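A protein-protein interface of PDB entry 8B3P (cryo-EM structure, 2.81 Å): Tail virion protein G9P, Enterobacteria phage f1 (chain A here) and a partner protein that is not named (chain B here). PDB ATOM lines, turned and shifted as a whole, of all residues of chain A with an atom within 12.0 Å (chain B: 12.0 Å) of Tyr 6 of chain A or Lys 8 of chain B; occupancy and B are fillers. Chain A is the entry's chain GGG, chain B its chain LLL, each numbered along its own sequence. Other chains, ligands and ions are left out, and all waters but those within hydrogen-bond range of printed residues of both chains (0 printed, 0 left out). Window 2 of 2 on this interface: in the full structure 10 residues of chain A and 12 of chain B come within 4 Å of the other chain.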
ATOM      1  N   MET A   1      -7.259  25.348   2.934  1.00  0.00           N
ATOM      2  CA  MET A   1      -8.118  24.119   3.072  1.00  0.00           C
ATOM      3  C   MET A   1      -7.449  23.102   4.000  1.00  0.00           C
ATOM      4  O   MET A   1      -7.764  21.907   3.968  1.00  0.00           O
ATOM      5  CB  MET A   1      -8.382  23.473   1.706  1.00  0.00           C
ATOM      6  CG  MET A   1      -9.211  24.328   0.745  1.00  0.00           C
ATOM      7  SD  MET A   1     -10.846  24.869   1.338  1.00  0.00           S
ATOM      8  CE  MET A   1     -11.689  23.301   1.542  1.00  0.00           C
ATOM      9  N   SER A   2      -6.538  23.607   4.839  1.00  0.00           N
ATOM     10  CA  SER A   2      -5.756  22.810   5.772  1.00  0.00           C
ATOM     11  C   SER A   2      -6.663  22.030   6.724  1.00  0.00           C
ATOM     12  O   SER A   2      -6.447  20.837   6.928  1.00  0.00           O
ATOM     13  CB  SER A   2      -4.770  23.672   6.519  1.00  0.00           C
ATOM     14  OG  SER A   2      -5.443  24.710   7.216  1.00  0.00           O
ATOM     15  N   VAL A   3      -7.685  22.707   7.272  1.00  0.00           N
ATOM     16  CA  VAL A   3      -8.601  22.125   8.247  1.00  0.00           C
ATOM     17  C   VAL A   3      -9.249  20.869   7.662  1.00  0.00           C
ATOM     18  O   VAL A   3      -9.191  19.806   8.280  1.00  0.00           O
ATOM     19  CB  VAL A   3      -9.658  23.132   8.750  1.00  0.00           C
ATOM     20  CG1 VAL A   3     -10.647  22.480   9.704  1.00  0.00           C
ATOM     21  CG2 VAL A   3      -9.024  24.352   9.404  1.00  0.00           C
ATOM     22  N   LEU A   4      -9.843  21.013   6.467  1.00  0.00           N
ATOM     23  CA  LEU A   4     -10.502  19.923   5.761  1.00  0.00           C
ATOM     24  C   LEU A   4      -9.530  18.756   5.577  1.00  0.00           C
ATOM     25  O   LEU A   4      -9.854  17.628   5.948  1.00  0.00           O
ATOM     26  CB  LEU A   4     -11.055  20.438   4.425  1.00  0.00           C
ATOM     27  CG  LEU A   4     -12.120  19.558   3.765  1.00  0.00           C
ATOM     28  CD1 LEU A   4     -13.309  20.386   3.308  1.00  0.00           C
ATOM     29  CD2 LEU A   4     -11.548  18.762   2.603  1.00  0.00           C
ATOM     30  N   VAL A   5      -8.332  19.049   5.047  1.00  0.00           N
ATOM     31  CA  VAL A   5      -7.340  18.037   4.713  1.00  0.00           C
ATOM     32  C   VAL A   5      -7.016  17.200   5.953  1.00  0.00           C
ATOM     33  O   VAL A   5      -7.029  15.972   5.885  1.00  0.00           O
ATOM     34  CB  VAL A   5      -6.088  18.657   4.055  1.00  0.00           C
ATOM     35  CG1 VAL A   5      -4.864  17.750   4.119  1.00  0.00           C
ATOM     36  CG2 VAL A   5      -6.363  19.073   2.615  1.00  0.00           C
ATOM     37  N   TYR A   6      -6.762  17.873   7.082  1.00  0.00           N
ATOM     38  CA  TYR A   6      -6.277  17.214   8.284  1.00  0.00           C
ATOM     39  C   TYR A   6      -7.405  16.586   9.102  1.00  0.00           C
ATOM     40  O   TYR A   6      -7.140  15.727   9.942  1.00  0.00           O
ATOM     41  CB  TYR A   6      -5.346  18.137   9.075  1.00  0.00           C
ATOM     42  CG  TYR A   6      -3.945  18.182   8.518  1.00  0.00           C
ATOM     43  CD1 TYR A   6      -3.070  17.121   8.704  1.00  0.00           C
ATOM     44  CD2 TYR A   6      -3.498  19.273   7.784  1.00  0.00           C
ATOM     45  CE1 TYR A   6      -1.783  17.145   8.186  1.00  0.00           C
ATOM     46  CE2 TYR A   6      -2.214  19.314   7.259  1.00  0.00           C
ATOM     47  CZ  TYR A   6      -1.353  18.247   7.461  1.00  0.00           C
ATOM     48  OH  TYR A   6      -0.085  18.277   6.950  1.00  0.00           O
ATOM     49  N   SER A   7      -8.654  17.006   8.864  1.00  0.00           N
ATOM     50  CA  SER A   7      -9.779  16.390   9.553  1.00  0.00           C
ATOM     51  C   SER A   7     -10.205  15.111   8.833  1.00  0.00           C
ATOM     52  O   SER A   7     -10.568  14.132   9.483  1.00  0.00           O
ATOM     53  CB  SER A   7     -10.923  17.349   9.750  1.00  0.00           C
ATOM     54  OG  SER A   7     -11.504  17.691   8.504  1.00  0.00           O
ATOM     55  N   PHE A   8     -10.140  15.130   7.493  1.00  0.00           N
ATOM     56  CA  PHE A   8     -10.405  13.954   6.676  1.00  0.00           C
ATOM     57  C   PHE A   8      -9.338  12.887   6.922  1.00  0.00           C
ATOM     58  O   PHE A   8      -9.661  11.707   7.039  1.00  0.00           O
ATOM     59  CB  PHE A   8     -10.555  14.330   5.198  1.00  0.00           C
ATOM     60  CG  PHE A   8     -11.014  13.207   4.300  1.00  0.00           C
ATOM     61  CD1 PHE A   8     -12.327  12.760   4.341  1.00  0.00           C
ATOM     62  CD2 PHE A   8     -10.135  12.591   3.414  1.00  0.00           C
ATOM     63  CE1 PHE A   8     -12.753  11.724   3.518  1.00  0.00           C
ATOM     64  CE2 PHE A   8     -10.560  11.551   2.598  1.00  0.00           C
ATOM     65  CZ  PHE A   8     -11.867  11.117   2.654  1.00  0.00           C
ATOM     66  N   ALA A   9      -8.071  13.321   7.025  1.00  0.00           N
ATOM     67  CA  ALA A   9      -6.953  12.437   7.323  1.00  0.00           C
ATOM     68  C   ALA A   9      -7.186  11.718   8.649  1.00  0.00           C
ATOM     69  O   ALA A   9      -6.734  10.589   8.826  1.00  0.00           O
ATOM     70  CB  ALA A   9      -5.662  13.213   7.354  1.00  0.00           C
ATOM     71  N   SER A  10      -7.916  12.379   9.557  1.00  0.00           N
ATOM     72  CA  SER A  10      -8.165  11.867  10.894  1.00  0.00           C
ATOM     73  C   SER A  10      -9.308  10.846  10.890  1.00  0.00           C
ATOM     74  O   SER A  10      -9.340   9.959  11.744  1.00  0.00           O
ATOM     75  CB  SER A  10      -8.359  13.006  11.874  1.00  0.00           C
ATOM     76  OG  SER A  10      -8.947  12.563  13.087  1.00  0.00           O
ATOM     77  N   PHE A  11     -10.224  10.952   9.912  1.00  0.00           N
ATOM     78  CA  PHE A  11     -11.281   9.966   9.729  1.00  0.00           C
ATOM     79  C   PHE A  11     -10.703   8.667   9.166  1.00  0.00           C
ATOM     80  O   PHE A  11     -11.052   7.584   9.630  1.00  0.00           O
ATOM     81  CB  PHE A  11     -12.440  10.534   8.900  1.00  0.00           C
ATOM     82  CG  PHE A  11     -13.476   9.526   8.462  1.00  0.00           C
ATOM     83  CD1 PHE A  11     -14.547   9.195   9.285  1.00  0.00           C
ATOM     84  CD2 PHE A  11     -13.386   8.904   7.219  1.00  0.00           C
ATOM     85  CE1 PHE A  11     -15.493   8.260   8.880  1.00  0.00           C
ATOM     86  CE2 PHE A  11     -14.334   7.972   6.813  1.00  0.00           C
ATOM     87  CZ  PHE A  11     -15.387   7.650   7.645  1.00  0.00           C
ATOM     88  N   VAL A  12      -9.808   8.789   8.180  1.00  0.00           N
ATOM     89  CA  VAL A  12      -9.241   7.651   7.472  1.00  0.00           C
ATOM     90  C   VAL A  12      -8.287   6.881   8.391  1.00  0.00           C
ATOM     91  O   VAL A  12      -8.099   5.680   8.207  1.00  0.00           O
ATOM     92  CB  VAL A  12      -8.597   8.084   6.136  1.00  0.00           C
ATOM     93  CG1 VAL A  12      -7.896   6.948   5.404  1.00  0.00           C
ATOM     94  CG2 VAL A  12      -9.614   8.742   5.214  1.00  0.00           C
ATOM     95  N   LEU A  13      -7.707   7.560   9.394  1.00  0.00           N
ATOM     96  CA  LEU A  13      -6.791   6.913  10.323  1.00  0.00           C
ATOM     97  C   LEU A  13      -7.566   5.966  11.240  1.00  0.00           C
ATOM     98  O   LEU A  13      -7.101   4.861  11.518  1.00  0.00           O
ATOM     99  CB  LEU A  13      -6.017   7.975  11.116  1.00  0.00           C
ATOM    100  CG  LEU A  13      -4.943   7.466  12.081  1.00  0.00           C
ATOM    101  CD1 LEU A  13      -3.642   7.159  11.352  1.00  0.00           C
ATOM    102  CD2 LEU A  13      -4.703   8.472  13.197  1.00  0.00           C
ATOM    103  N   GLY A  14      -8.754   6.409  11.674  1.00  0.00           N
ATOM    104  CA  GLY A  14      -9.618   5.657  12.570  1.00  0.00           C
ATOM    105  C   GLY A  14     -10.286   4.472  11.877  1.00  0.00           C
ATOM    106  O   GLY A  14     -10.527   3.451  12.520  1.00  0.00           O
ATOM    107  N   TRP A  15     -10.585   4.631  10.576  1.00  0.00           N
ATOM    108  CA  TRP A  15     -11.180   3.581   9.755  1.00  0.00           C
ATOM    109  C   TRP A  15     -10.198   2.420   9.580  1.00  0.00           C
ATOM    110  O   TRP A  15     -10.600   1.260   9.647  1.00  0.00           O
ATOM    111  CB  TRP A  15     -11.718   4.127   8.416  1.00  0.00           C
ATOM    112  CG  TRP A  15     -12.317   3.083   7.516  1.00  0.00           C
ATOM    113  CD1 TRP A  15     -13.593   2.593   7.550  1.00  0.00           C
ATOM    114  CD2 TRP A  15     -11.654   2.385   6.444  1.00  0.00           C
ATOM    115  NE1 TRP A  15     -13.768   1.639   6.583  1.00  0.00           N
ATOM    116  CE2 TRP A  15     -12.595   1.485   5.891  1.00  0.00           C
ATOM    117  CE3 TRP A  15     -10.360   2.426   5.901  1.00  0.00           C
ATOM    118  CZ2 TRP A  15     -12.275   0.641   4.825  1.00  0.00           C
ATOM    119  CZ3 TRP A  15     -10.043   1.585   4.855  1.00  0.00           C
ATOM    120  CH2 TRP A  15     -10.992   0.710   4.321  1.00  0.00           C
ATOM    121  N   ASP B   5       1.493  25.207  11.072  1.00  0.00           N
ATOM    122  CA  ASP B   5      -0.001  25.223  11.017  1.00  0.00           C
ATOM    123  C   ASP B   5      -0.558  24.682  12.331  1.00  0.00           C
ATOM    124  O   ASP B   5      -0.034  23.701  12.857  1.00  0.00           O
ATOM    125  CB  ASP B   5      -0.546  24.385   9.855  1.00  0.00           C
ATOM    126  CG  ASP B   5      -0.077  24.805   8.468  1.00  0.00           C
ATOM    127  OD1 ASP B   5       0.108  26.022   8.243  1.00  0.00           O
ATOM    128  OD2 ASP B   5       0.085  23.908   7.611  1.00  0.00           O
ATOM    129  N   PRO B   6      -1.642  25.279  12.892  1.00  0.00           N
ATOM    130  CA  PRO B   6      -2.217  24.810  14.156  1.00  0.00           C
ATOM    131  C   PRO B   6      -2.866  23.433  14.019  1.00  0.00           C
ATOM    132  O   PRO B   6      -2.892  22.667  14.984  1.00  0.00           O
ATOM    133  CB  PRO B   6      -3.263  25.878  14.516  1.00  0.00           C
ATOM    134  CG  PRO B   6      -3.633  26.512  13.192  1.00  0.00           C
ATOM    135  CD  PRO B   6      -2.379  26.432  12.343  1.00  0.00           C
ATOM    136  N   ALA B   7      -3.342  23.140  12.801  1.00  0.00           N
ATOM    137  CA  ALA B   7      -4.121  21.951  12.480  1.00  0.00           C
ATOM    138  C   ALA B   7      -3.212  20.760  12.181  1.00  0.00           C
ATOM    139  O   ALA B   7      -3.542  19.628  12.539  1.00  0.00           O
ATOM    140  CB  ALA B   7      -5.049  22.239  11.327  1.00  0.00           C
ATOM    141  N   LYS B   8      -2.050  21.026  11.566  1.00  0.00           N
ATOM    142  CA  LYS B   8      -1.043  19.991  11.383  1.00  0.00           C
ATOM    143  C   LYS B   8      -0.580  19.488  12.750  1.00  0.00           C
ATOM    144  O   LYS B   8      -0.492  18.281  12.955  1.00  0.00           O
ATOM    145  CB  LYS B   8       0.129  20.468  10.522  1.00  0.00           C
ATOM    146  CG  LYS B   8       1.204  19.420  10.272  1.00  0.00           C
ATOM    147  CD  LYS B   8       2.439  19.967   9.615  1.00  0.00           C
ATOM    148  CE  LYS B   8       3.557  18.951   9.583  1.00  0.00           C
ATOM    149  NZ  LYS B   8       4.706  19.448   8.793  1.00  0.00           N
ATOM    150  N   ALA B   9      -0.312  20.425  13.672  1.00  0.00           N
ATOM    151  CA  ALA B   9       0.095  20.130  15.040  1.00  0.00           C
ATOM    152  C   ALA B   9      -0.940  19.250  15.743  1.00  0.00           C
ATOM    153  O   ALA B   9      -0.574  18.274  16.403  1.00  0.00           O
ATOM    154  CB  ALA B   9       0.346  21.414  15.796  1.00  0.00           C
ATOM    155  N   ALA B  10      -2.226  19.597  15.572  1.00  0.00           N
ATOM    156  CA  ALA B  10      -3.349  18.875  16.155  1.00  0.00           C
ATOM    157  C   ALA B  10      -3.334  17.410  15.721  1.00  0.00           C
ATOM    158  O   ALA B  10      -3.400  16.526  16.568  1.00  0.00           O
ATOM    159  CB  ALA B  10      -4.657  19.546  15.806  1.00  0.00           C
ATOM    160  N   PHE B  11      -3.229  17.170  14.408  1.00  0.00           N
ATOM    161  CA  PHE B  11      -3.248  15.823  13.859  1.00  0.00           C
ATOM    162  C   PHE B  11      -2.055  15.016  14.375  1.00  0.00           C
ATOM    163  O   PHE B  11      -2.199  13.832  14.656  1.00  0.00           O
ATOM    164  CB  PHE B  11      -3.351  15.859  12.331  1.00  0.00           C
ATOM    165  CG  PHE B  11      -3.225  14.519  11.650  1.00  0.00           C
ATOM    166  CD1 PHE B  11      -4.256  13.585  11.698  1.00  0.00           C
ATOM    167  CD2 PHE B  11      -2.076  14.193  10.941  1.00  0.00           C
ATOM    168  CE1 PHE B  11      -4.126  12.348  11.081  1.00  0.00           C
ATOM    169  CE2 PHE B  11      -1.949  12.958  10.320  1.00  0.00           C
ATOM    170  CZ  PHE B  11      -2.972  12.036  10.392  1.00  0.00           C
ATOM    171  N   ASP B  12      -0.890  15.663  14.509  1.00  0.00           N
ATOM    172  CA  ASP B  12       0.323  14.989  14.951  1.00  0.00           C
ATOM    173  C   ASP B  12       0.167  14.475  16.381  1.00  0.00           C
ATOM    174  O   ASP B  12       0.609  13.368  16.688  1.00  0.00           O
ATOM    175  CB  ASP B  12       1.562  15.875  14.801  1.00  0.00           C
ATOM    176  CG  ASP B  12       1.940  16.166  13.357  1.00  0.00           C
ATOM    177  OD1 ASP B  12       1.462  15.443  12.455  1.00  0.00           O
ATOM    178  OD2 ASP B  12       2.714  17.117  13.141  1.00  0.00           O
ATOM    179  N   SER B  13      -0.478  15.274  17.239  1.00  0.00           N
ATOM    180  CA  SER B  13      -0.677  14.901  18.632  1.00  0.00           C
ATOM    181  C   SER B  13      -1.668  13.740  18.748  1.00  0.00           C
ATOM    182  O   SER B  13      -1.469  12.836  19.567  1.00  0.00           O
ATOM    183  CB  SER B  13      -1.096  16.087  19.459  1.00  0.00           C
ATOM    184  OG  SER B  13      -2.484  16.336  19.312  1.00  0.00           O
ATOM    185  N   LEU B  14      -2.719  13.786  17.910  1.00  0.00           N
ATOM    186  CA  LEU B  14      -3.754  12.767  17.871  1.00  0.00           C
ATOM    187  C   LEU B  14      -3.131  11.421  17.535  1.00  0.00           C
ATOM    188  O   LEU B  14      -3.510  10.454  18.167  1.00  0.00           O
ATOM    189  CB  LEU B  14      -4.868  13.103  16.866  1.00  0.00           C
ATOM    190  CG  LEU B  14      -5.908  11.991  16.666  1.00  0.00           C
ATOM    191  CD1 LEU B  14      -6.916  11.936  17.808  1.00  0.00           C
ATOM    192  CD2 LEU B  14      -6.607  12.066  15.314  1.00  0.00           C
ATOM    193  N   GLN B  15      -2.222  11.380  16.548  1.00  0.00           N
ATOM    194  CA  GLN B  15      -1.626  10.138  16.078  1.00  0.00           C
ATOM    195  C   GLN B  15      -0.992   9.371  17.236  1.00  0.00           C
ATOM    196  O   GLN B  15      -1.135   8.151  17.288  1.00  0.00           O
ATOM    197  CB  GLN B  15      -0.600  10.370  14.965  1.00  0.00           C
ATOM    198  CG  GLN B  15      -1.202  10.515  13.573  1.00  0.00           C
ATOM    199  CD  GLN B  15      -0.331   9.909  12.496  1.00  0.00           C
ATOM    200  OE1 GLN B  15       0.300  10.613  11.710  1.00  0.00           O
ATOM    201  NE2 GLN B  15      -0.279   8.586  12.460  1.00  0.00           N
ATOM    202  N   ALA B  16      -0.300  10.091  18.138  1.00  0.00           N
ATOM    203  CA  ALA B  16       0.411   9.457  19.246  1.00  0.00           C
ATOM    204  C   ALA B  16      -0.551   8.735  20.199  1.00  0.00           C
ATOM    205  O   ALA B  16      -0.345   7.565  20.556  1.00  0.00           O
ATOM    206  CB  ALA B  16       1.272  10.471  19.965  1.00  0.00           C
ATOM    207  N   SER B  17      -1.613   9.454  20.590  1.00  0.00           N
ATOM    208  CA  SER B  17      -2.628   8.951  21.503  1.00  0.00           C
ATOM    209  C   SER B  17      -3.340   7.734  20.910  1.00  0.00           C
ATOM    210  O   SER B  17      -3.596   6.771  21.626  1.00  0.00           O
ATOM    211  CB  SER B  17      -3.601  10.043  21.882  1.00  0.00           C
ATOM    212  OG  SER B  17      -4.497  10.330  20.815  1.00  0.00           O
ATOM    213  N   ALA B  18      -3.629   7.790  19.599  1.00  0.00           N
ATOM    214  CA  ALA B  18      -4.344   6.739  18.891  1.00  0.00           C
ATOM    215  C   ALA B  18      -3.507   5.468  18.836  1.00  0.00           C
ATOM    216  O   ALA B  18      -4.073   4.386  18.935  1.00  0.00           O
ATOM    217  CB  ALA B  18      -4.737   7.185  17.505  1.00  0.00           C
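No residue of chain B comes within 4 Å of Ser 2 of chain A. No residue of chain B comes within 4 Å of Val 3 of chain A. No residue of chain B comes within 4 Å of Val 5 of chain A. Of chain B, only Lys 8 (3.7 Å) and Phe 11 (3.8 Å) come within 4 Å of Tyr 6 of chain A. No residue of chain B comes within 4 Å of Ser 7 of chain A. Ala 9 of chain A touches just one residue of chain B: Phe 11. Of chain B, only Leu 14 comes within 4 Å of Ser 10 of chain A. Gly 14 of chain A touches none of the printed residues of chain B. Asp 5 of chain B touches none of the printed residues of chain A. Ala 7 of chain B touches none of the printed residues of chain A. Lys 8 of chain B touches just one residue of chain A: Tyr 6. No residue of chain A comes within 4 Å of Ala 9 of chain B. No residue of chain A comes within 4 Å of Ala 10 of chain B. Printed residues of chain A within 4 Å of Leu 14 of chain B: Ser 10 (3.3 Å). Of the printed residues of chain A, Gln 15 of chain B touches Leu 13 (3.8 Å). The nearest residue of chain B that does not touch Tyr 6 of chain A is Ala 7 of chain B (4.2 Å). The nearest residue of chain A that does not touch Lys 8 of chain B is Ser 2 of chain A (6.3 Å). The nearest printed residue of chain A that does not touch Gln 15 of chain B is Ala 9 of chain A (7.3 Å).
Hydrophobic or aromatic side chains of chain B that line the printed part of chain A: Phe 11 and Leu 14. Among the printed residues, no Asp or Glu carboxylate lies within 4 Å of a Lys or Arg side-chain nitrogen of the other chain.
The side-chain hydroxyl of Ser 17 of chain B is in hydrogen-bond range of the backbone carbonyl oxygen of Leu 14 of chain B, 2.8 Å away.
Among the printed residues, merely in contact across the chains: Tyr 6 of chain A with Lys 8 of chain B (3.7 Å), Tyr 6 of chain A with Phe 11 of chain B (3.8 Å), Ala 9 of chain A with Phe 11 of chain B (3.9 Å), Ser 10 of chain A with Leu 14 of chain B (3.3 Å) and Leu 13 of chain A with Gln 15 of chain B (3.8 Å).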
